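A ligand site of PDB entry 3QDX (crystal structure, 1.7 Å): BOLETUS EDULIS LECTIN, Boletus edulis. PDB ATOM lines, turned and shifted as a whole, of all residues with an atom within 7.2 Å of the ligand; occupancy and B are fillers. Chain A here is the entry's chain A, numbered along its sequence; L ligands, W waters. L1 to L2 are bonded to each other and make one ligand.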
ATOM      1  N   PHE A  27      -2.605  28.269  10.792  1.00  0.00           N
ATOM      2  CA  PHE A  27      -2.692  27.203  11.776  1.00  0.00           C
ATOM      3  C   PHE A  27      -1.330  26.984  12.506  1.00  0.00           C
ATOM      4  O   PHE A  27      -0.264  27.349  11.982  1.00  0.00           O
ATOM      5  CB  PHE A  27      -3.246  25.920  11.117  1.00  0.00           C
ATOM      6  CG  PHE A  27      -3.748  24.917  12.109  1.00  0.00           C
ATOM      7  CD1 PHE A  27      -3.069  23.722  12.291  1.00  0.00           C
ATOM      8  CD2 PHE A  27      -4.870  25.180  12.868  1.00  0.00           C
ATOM      9  CE1 PHE A  27      -3.511  22.789  13.232  1.00  0.00           C
ATOM     10  CE2 PHE A  27      -5.331  24.259  13.798  1.00  0.00           C
ATOM     11  CZ  PHE A  27      -4.648  23.069  13.988  1.00  0.00           C
ATOM     12  N   HIS A  28      -1.391  26.456  13.734  1.00  0.00           N
ATOM     13  CA  HIS A  28      -0.276  26.503  14.671  1.00  0.00           C
ATOM     14  C   HIS A  28       0.738  25.343  14.557  1.00  0.00           C
ATOM     15  O   HIS A  28       1.759  25.343  15.221  1.00  0.00           O
ATOM     16  CB  HIS A  28      -0.814  26.617  16.114  1.00  0.00           C
ATOM     17  CG  HIS A  28      -1.488  25.375  16.623  1.00  0.00           C
ATOM     18  ND1 HIS A  28      -2.850  25.175  16.539  1.00  0.00           N
ATOM     19  CD2 HIS A  28      -0.983  24.294  17.250  1.00  0.00           C
ATOM     20  CE1 HIS A  28      -3.150  24.006  17.070  1.00  0.00           C
ATOM     21  NE2 HIS A  28      -2.030  23.444  17.498  1.00  0.00           N
ATOM     22  N   TYR A  29       0.464  24.348  13.715  1.00  0.00           N
ATOM     23  CA  TYR A  29       1.445  23.275  13.545  1.00  0.00           C
ATOM     24  C   TYR A  29       2.665  23.761  12.749  1.00  0.00           C
ATOM     25  O   TYR A  29       2.624  24.811  12.108  1.00  0.00           O
ATOM     26  CB  TYR A  29       0.809  22.133  12.776  1.00  0.00           C
ATOM     27  CG  TYR A  29      -0.194  21.272  13.543  1.00  0.00           C
ATOM     28  CD1 TYR A  29      -0.952  20.316  12.860  1.00  0.00           C
ATOM     29  CD2 TYR A  29      -0.402  21.420  14.912  1.00  0.00           C
ATOM     30  CE1 TYR A  29      -1.859  19.524  13.510  1.00  0.00           C
ATOM     31  CE2 TYR A  29      -1.344  20.618  15.584  1.00  0.00           C
ATOM     32  CZ  TYR A  29      -2.047  19.671  14.870  1.00  0.00           C
ATOM     33  OH  TYR A  29      -2.970  18.848  15.509  1.00  0.00           O
ATOM     34  N   ALA A  30       3.735  22.977  12.782  1.00  0.00           N
ATOM     35  CA  ALA A  30       4.910  23.221  11.938  1.00  0.00           C
ATOM     36  C   ALA A  30       5.490  24.602  12.195  1.00  0.00           C
ATOM     37  O   ALA A  30       5.961  25.262  11.282  1.00  0.00           O
ATOM     38  CB  ALA A  30       4.584  23.044  10.449  1.00  0.00           C
ATOM     39  N   ASN A  31       5.481  25.004  13.468  1.00  0.00           N
ATOM     40  CA  ASN A  31       6.031  26.301  13.886  1.00  0.00           C
ATOM     41  C   ASN A  31       5.283  27.501  13.279  1.00  0.00           C
ATOM     42  O   ASN A  31       5.828  28.594  13.165  1.00  0.00           O
ATOM     43  CB  ASN A  31       7.545  26.377  13.647  1.00  0.00           C
ATOM     44  CG  ASN A  31       8.315  25.417  14.547  1.00  0.00           C
ATOM     45  OD1 ASN A  31       8.075  25.362  15.745  1.00  0.00           O
ATOM     46  ND2 ASN A  31       9.203  24.646  13.956  1.00  0.00           N
ATOM     47  N   GLY A  32       4.032  27.264  12.910  1.00  0.00           N
ATOM     48  CA  GLY A  32       3.161  28.337  12.421  1.00  0.00           C
ATOM     49  C   GLY A  32       3.619  28.925  11.097  1.00  0.00           C
ATOM     50  O   GLY A  32       4.084  28.228  10.186  1.00  0.00           O
ATOM     51  N   GLY A  47       6.605  27.225   8.706  1.00  0.00           N
ATOM     52  CA  GLY A  47       7.835  26.721   9.316  1.00  0.00           C
ATOM     53  C   GLY A  47       8.260  25.336   8.891  1.00  0.00           C
ATOM     54  O   GLY A  47       9.356  24.892   9.224  1.00  0.00           O
ATOM     55  N   GLY A  48       7.395  24.640   8.147  1.00  0.00           N
ATOM     56  CA  GLY A  48       7.688  23.291   7.694  1.00  0.00           C
ATOM     57  C   GLY A  48       6.481  22.703   7.011  1.00  0.00           C
ATOM     58  O   GLY A  48       5.491  23.407   6.789  1.00  0.00           O
ATOM     59  N   SER A  49       6.560  21.421   6.640  1.00  0.00           N
ATOM     60  CA  SER A  49       5.356  20.737   6.150  1.00  0.00           C
ATOM     61  C   SER A  49       4.432  20.430   7.332  1.00  0.00           C
ATOM     62  O   SER A  49       4.922  20.087   8.424  1.00  0.00           O
ATOM     63  CB  SER A  49       5.728  19.420   5.431  1.00  0.00           C
ATOM     64  OG  SER A  49       4.562  18.685   5.074  1.00  0.00           O
ATOM     65  N   GLY A  50       3.125  20.568   7.110  1.00  0.00           N
ATOM     66  CA  GLY A  50       2.093  20.080   8.065  1.00  0.00           C
ATOM     67  C   GLY A  50       1.198  21.166   8.640  1.00  0.00           C
ATOM     68  O   GLY A  50       0.524  20.962   9.650  1.00  0.00           O
ATOM     69  N   THR A  51       1.213  22.342   8.043  1.00  0.00           N
ATOM     70  CA  THR A  51       0.316  23.399   8.470  1.00  0.00           C
ATOM     71  C   THR A  51      -0.311  24.117   7.266  1.00  0.00           C
ATOM     72  O   THR A  51      -0.194  23.646   6.119  1.00  0.00           O
ATOM     73  CB  THR A  51       0.984  24.378   9.464  1.00  0.00           C
ATOM     74  OG1 THR A  51      -0.031  25.111  10.165  1.00  0.00           O
ATOM     75  CG2 THR A  51       1.945  25.377   8.727  1.00  0.00           C
ATOM     76  N   VAL A  71       0.617  22.675   3.252  1.00  0.00           N
ATOM     77  CA  VAL A  71       1.416  21.532   2.825  1.00  0.00           C
ATOM     78  C   VAL A  71       1.159  20.357   3.768  1.00  0.00           C
ATOM     79  O   VAL A  71       1.239  20.498   4.981  1.00  0.00           O
ATOM     80  CB  VAL A  71       2.885  21.890   2.739  1.00  0.00           C
ATOM     81  CG1 VAL A  71       3.680  20.674   2.209  1.00  0.00           C
ATOM     82  CG2 VAL A  71       3.080  23.095   1.806  1.00  0.00           C
ATOM     83  N   HIS A  72       0.803  19.201   3.215  1.00  0.00           N
ATOM     84  CA  HIS A  72       0.544  18.008   4.040  1.00  0.00           C
ATOM     85  C   HIS A  72       1.477  16.898   3.581  1.00  0.00           C
ATOM     86  O   HIS A  72       1.436  16.499   2.419  1.00  0.00           O
ATOM     87  CB  HIS A  72      -0.905  17.536   3.871  1.00  0.00           C
ATOM     88  CG  HIS A  72      -1.196  16.260   4.600  1.00  0.00           C
ATOM     89  ND1 HIS A  72      -1.570  15.093   3.946  1.00  0.00           N
ATOM     90  CD2 HIS A  72      -1.128  15.950   5.917  1.00  0.00           C
ATOM     91  CE1 HIS A  72      -1.743  14.127   4.850  1.00  0.00           C
ATOM     92  NE2 HIS A  72      -1.490  14.629   6.049  1.00  0.00           N
ATOM     93  N   ASN A  73       2.307  16.408   4.484  1.00  0.00           N
ATOM     94  CA  ASN A  73       3.278  15.370   4.126  1.00  0.00           C
ATOM     95  C   ASN A  73       4.062  15.717   2.851  1.00  0.00           C
ATOM     96  O   ASN A  73       4.215  14.908   1.930  1.00  0.00           O
ATOM     97  CB  ASN A  73       2.599  13.984   4.061  1.00  0.00           C
ATOM     98  CG  ASN A  73       2.204  13.461   5.441  1.00  0.00           C
ATOM     99  OD1 ASN A  73       2.760  13.882   6.450  1.00  0.00           O
ATOM    100  ND2 ASN A  73       1.250  12.518   5.476  1.00  0.00           N
ATOM    101  N   TYR A  74       4.576  16.951   2.825  1.00  0.00           N
ATOM    102  CA  TYR A  74       5.474  17.446   1.773  1.00  0.00           C
ATOM    103  C   TYR A  74       4.819  17.639   0.419  1.00  0.00           C
ATOM    104  O   TYR A  74       5.506  17.820  -0.581  1.00  0.00           O
ATOM    105  CB  TYR A  74       6.738  16.550   1.661  1.00  0.00           C
ATOM    106  CG  TYR A  74       7.293  16.260   3.035  1.00  0.00           C
ATOM    107  CD1 TYR A  74       7.062  15.046   3.655  1.00  0.00           C
ATOM    108  CD2 TYR A  74       7.997  17.242   3.725  1.00  0.00           C
ATOM    109  CE1 TYR A  74       7.549  14.802   4.940  1.00  0.00           C
ATOM    110  CE2 TYR A  74       8.493  16.993   5.009  1.00  0.00           C
ATOM    111  CZ  TYR A  74       8.254  15.771   5.599  1.00  0.00           C
ATOM    112  OH  TYR A  74       8.724  15.545   6.867  1.00  0.00           O
ATOM    113  N   LYS A  75       3.483  17.621   0.368  1.00  0.00           N
ATOM    114  CA  LYS A  75       2.782  17.920  -0.880  1.00  0.00           C
ATOM    115  C   LYS A  75       1.751  19.011  -0.647  1.00  0.00           C
ATOM    116  O   LYS A  75       1.113  19.030   0.402  1.00  0.00           O
ATOM    117  CB  LYS A  75       2.064  16.681  -1.415  1.00  0.00           C
ATOM    118  CG  LYS A  75       2.998  15.516  -1.761  1.00  0.00           C
ATOM    119  CD  LYS A  75       2.214  14.440  -2.452  1.00  0.00           C
ATOM    120  CE  LYS A  75       3.107  13.240  -2.729  1.00  0.00           C
ATOM    121  NZ  LYS A  75       2.376  12.216  -3.546  1.00  0.00           N
ATOM    122  N   TYR A  97      -9.710  21.501   9.512  1.00  0.00           N
ATOM    123  CA  TYR A  97      -8.900  20.616   8.672  1.00  0.00           C
ATOM    124  C   TYR A  97      -8.028  19.700   9.508  1.00  0.00           C
ATOM    125  O   TYR A  97      -7.325  18.858   8.961  1.00  0.00           O
ATOM    126  CB  TYR A  97      -8.034  21.434   7.714  1.00  0.00           C
ATOM    127  CG  TYR A  97      -8.835  22.200   6.701  1.00  0.00           C
ATOM    128  CD1 TYR A  97      -9.189  23.536   6.919  1.00  0.00           C
ATOM    129  CD2 TYR A  97      -9.274  21.580   5.539  1.00  0.00           C
ATOM    130  CE1 TYR A  97      -9.961  24.247   5.982  1.00  0.00           C
ATOM    131  CE2 TYR A  97     -10.016  22.261   4.595  1.00  0.00           C
ATOM    132  CZ  TYR A  97     -10.371  23.597   4.814  1.00  0.00           C
ATOM    133  OH  TYR A  97     -11.132  24.238   3.879  1.00  0.00           O
ATOM    134  N   TYR A  98      -8.069  19.858  10.832  1.00  0.00           N
ATOM    135  CA  TYR A  98      -7.178  19.110  11.713  1.00  0.00           C
ATOM    136  C   TYR A  98      -7.950  18.476  12.865  1.00  0.00           C
ATOM    137  O   TYR A  98      -9.142  18.684  12.982  1.00  0.00           O
ATOM    138  CB  TYR A  98      -6.096  20.030  12.268  1.00  0.00           C
ATOM    139  CG  TYR A  98      -5.276  20.682  11.159  1.00  0.00           C
ATOM    140  CD1 TYR A  98      -5.610  21.929  10.625  1.00  0.00           C
ATOM    141  CD2 TYR A  98      -4.187  20.012  10.613  1.00  0.00           C
ATOM    142  CE1 TYR A  98      -4.857  22.508   9.609  1.00  0.00           C
ATOM    143  CE2 TYR A  98      -3.413  20.590   9.588  1.00  0.00           C
ATOM    144  CZ  TYR A  98      -3.753  21.835   9.097  1.00  0.00           C
ATOM    145  OH  TYR A  98      -3.006  22.401   8.080  1.00  0.00           O
ATOM    146  N   ASN A  99      -7.237  17.720  13.692  1.00  0.00           N
ATOM    147  CA  ASN A  99      -7.814  17.066  14.871  1.00  0.00           C
ATOM    148  C   ASN A  99      -9.086  16.284  14.557  1.00  0.00           C
ATOM    149  O   ASN A  99     -10.084  16.369  15.288  1.00  0.00           O
ATOM    150  CB  ASN A  99      -8.053  18.078  15.994  1.00  0.00           C
ATOM    151  CG  ASN A  99      -6.747  18.719  16.477  1.00  0.00           C
ATOM    152  OD1 ASN A  99      -5.955  18.075  17.166  1.00  0.00           O
ATOM    153  ND2 ASN A  99      -6.508  19.972  16.100  1.00  0.00           N
ATOM    154  N   ASN A 100      -9.027  15.543  13.452  1.00  0.00           N
ATOM    155  CA  ASN A 100     -10.154  14.742  12.953  1.00  0.00           C
ATOM    156  C   ASN A 100     -11.404  15.576  12.661  1.00  0.00           C
ATOM    157  O   ASN A 100     -12.530  15.070  12.752  1.00  0.00           O
ATOM    158  CB  ASN A 100     -10.469  13.600  13.926  1.00  0.00           C
ATOM    159  CG  ASN A 100      -9.350  12.577  14.020  1.00  0.00           C
ATOM    160  OD1 ASN A 100      -8.689  12.263  13.018  1.00  0.00           O
ATOM    161  ND2 ASN A 100      -9.123  12.052  15.215  1.00  0.00           N
ATOM    162  N   ALA A 104     -10.860  17.565   7.264  1.00  0.00           N
ATOM    163  CA  ALA A 104      -9.523  16.934   7.159  1.00  0.00           C
ATOM    164  C   ALA A 104      -9.376  16.123   5.880  1.00  0.00           C
ATOM    165  O   ALA A 104      -8.294  16.083   5.272  1.00  0.00           O
ATOM    166  CB  ALA A 104      -9.231  16.047   8.389  1.00  0.00           C
ATOM    167  N   ARG A 107      -7.784  18.127   3.054  1.00  0.00           N
ATOM    168  CA  ARG A 107      -6.343  18.287   3.205  1.00  0.00           C
ATOM    169  C   ARG A 107      -5.602  17.021   2.785  1.00  0.00           C
ATOM    170  O   ARG A 107      -4.561  17.073   2.122  1.00  0.00           O
ATOM    171  CB  ARG A 107      -5.984  18.684   4.646  1.00  0.00           C
ATOM    172  CG  ARG A 107      -4.493  18.518   4.995  1.00  0.00           C
ATOM    173  CD  ARG A 107      -4.198  18.996   6.424  1.00  0.00           C
ATOM    174  NE  ARG A 107      -5.001  18.293   7.432  1.00  0.00           N
ATOM    175  CZ  ARG A 107      -4.779  17.048   7.873  1.00  0.00           C
ATOM    176  NH1 ARG A 107      -3.771  16.331   7.397  1.00  0.00           N
ATOM    177  NH2 ARG A 107      -5.583  16.493   8.767  1.00  0.00           N
ATOM    178  N   GLU A 108      -6.173  15.871   3.157  1.00  0.00           N
ATOM    179  CA  GLU A 108      -5.491  14.610   2.942  1.00  0.00           C
ATOM    180  C   GLU A 108      -5.392  14.269   1.458  1.00  0.00           C
ATOM    181  O   GLU A 108      -4.495  13.538   1.030  1.00  0.00           O
ATOM    182  CB  GLU A 108      -6.169  13.501   3.765  1.00  0.00           C
ATOM    183  CG  GLU A 108      -5.879  13.624   5.255  1.00  0.00           C
ATOM    184  CD  GLU A 108      -6.793  12.799   6.137  1.00  0.00           C
ATOM    185  OE1 GLU A 108      -7.820  12.275   5.638  1.00  0.00           O
ATOM    186  OE2 GLU A 108      -6.480  12.684   7.338  1.00  0.00           O
HETATM  187  O1  LIG L   1      -0.534  15.717   9.140  1.00  0.00           O
HETATM  188  C1  LIG L   1       0.847  15.323   8.852  1.00  0.00           C
HETATM  189  O2  LIG L   1       1.235  14.129   9.585  1.00  0.00           O
HETATM  190  C2  LIG L   1       1.764  16.506   9.165  1.00  0.00           C
HETATM  191  N1  LIG L   1       3.183  16.174   8.934  1.00  0.00           N
HETATM  192  C3  LIG L   1       1.561  16.969  10.603  1.00  0.00           C
HETATM  193  O3  LIG L   1       2.350  18.136  10.778  1.00  0.00           O
HETATM  194  C4  LIG L   1       0.088  17.302  10.844  1.00  0.00           C
HETATM  195  O4  LIG L   1      -0.335  18.372   9.966  1.00  0.00           O
HETATM  196  C5  LIG L   1      -0.759  16.090  10.494  1.00  0.00           C
HETATM  197  C6  LIG L   1      -2.257  16.494  10.711  1.00  0.00           C
HETATM  198  O5  LIG L   1      -3.063  15.295  10.605  1.00  0.00           O
HETATM  199  C7  LIG L   1       3.843  16.624   7.855  1.00  0.00           C
HETATM  200  O6  LIG L   1       3.365  17.326   6.968  1.00  0.00           O
HETATM  201  C8  LIG L   1       5.324  16.188   7.784  1.00  0.00           C
HETATM  202  C1  LG2 L   2       3.161  18.132  11.956  1.00  0.00           C
HETATM  203  C2  LG2 L   2       4.164  19.287  11.936  1.00  0.00           C
HETATM  204  C3  LG2 L   2       4.888  19.329  13.292  1.00  0.00           C
HETATM  205  C4  LG2 L   2       3.864  19.413  14.412  1.00  0.00           C
HETATM  206  C5  LG2 L   2       2.828  18.301  14.276  1.00  0.00           C
HETATM  207  C6  LG2 L   2       1.734  18.518  15.313  1.00  0.00           C
HETATM  208  O1  LG2 L   2       5.088  19.069  10.889  1.00  0.00           O
HETATM  209  O2  LG2 L   2       5.803  20.410  13.388  1.00  0.00           O
HETATM  210  O3  LG2 L   2       3.181  20.668  14.475  1.00  0.00           O
HETATM  211  O4  LG2 L   2       2.217  18.290  12.989  1.00  0.00           O
HETATM  212  O5  LG2 L   2       1.096  17.278  15.518  1.00  0.00           O
HETATM  213  O   HOH W   1      -0.916  18.434   7.269  1.00  0.00           O
HETATM  214  O   HOH W   2       2.829  21.627  17.059  1.00  0.00           O
HETATM  215  O   HOH W   3       4.514  14.366  10.937  1.00  0.00           O
HETATM  216  O   HOH W   4      -3.918  13.689   8.182  1.00  0.00           O
HETATM  217  O   HOH W   5       6.933  17.028  11.281  1.00  0.00           O
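N of Asn 73 is in hydrogen-bond range of O6 of LIG L1 (2.9 Å). O of Ser 49 lies within hydrogen-bond range of O1 of LG2 L2. The backbone carbonyl oxygen (O) of Gly 50 lies within hydrogen-bond range of an oxygen (O4) of LIG L1 (2.7 Å). N of Gly 50 lies close to O6 of LIG L1 (3.3 Å). An oxygen (O6) of LIG L1 is in hydrogen-bond range of the side-chain hydroxyl of Ser 49 (2.6 Å). The side-chain amide oxygen (OD1) of Asn 73 lies close to a nitrogen (N1) of LIG L1 (3.4 Å). The guanidinium group (NH2) of Arg 107 sits at hydrogen-bond distance from an oxygen (O5) of LIG L1 (3.3 Å). A ring nitrogen (NE2) of His 72 lies close to an oxygen (O1) of LIG L1, at 3.4 Å. The backbone NH (N) of Ala 30 is in hydrogen-bond range of an oxygen (O3) of LG2 L2, 2.9 Å away.
NE of Arg 107 is in hydrogen-bond range of O of Tyr 97. The backbone NH of Gly 47 sits close to the backbone carbonyl oxygen of Ala 30. A ring nitrogen (NE2) of His 72 lies close to the guanidinium group (NH1) of Arg 107 (3.1 Å). The backbone carbonyl oxygen of Tyr 29 sits close to the side-chain hydroxyl of Thr 51, at 3.3 Å. The side-chain hydroxyl (OG) of Ser 49 lies within hydrogen-bond range of the backbone NH (N) of Tyr 74 (2.8 Å). The backbone carbonyl oxygen (O) of Val 71 is in hydrogen-bond range of the backbone NH (N) of Gly 50 (2.8 Å). The side-chain hydroxyl of Ser 49 is in hydrogen-bond range of the backbone NH of Asn 73, 3.3 Å away.
Merely in contact with the ligand: Tyr 29 (3.3 Å), Tyr 74 (3.6 Å) and Tyr 98 (3.8 Å).
Water W4 lies within hydrogen-bond range of NH1 of Arg 107 (2.8 Å), OE2 of Glu 108 (2.9 Å), O5 of LIG L1 (3.0 Å) and NE2 of His 72 (3.4 Å).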
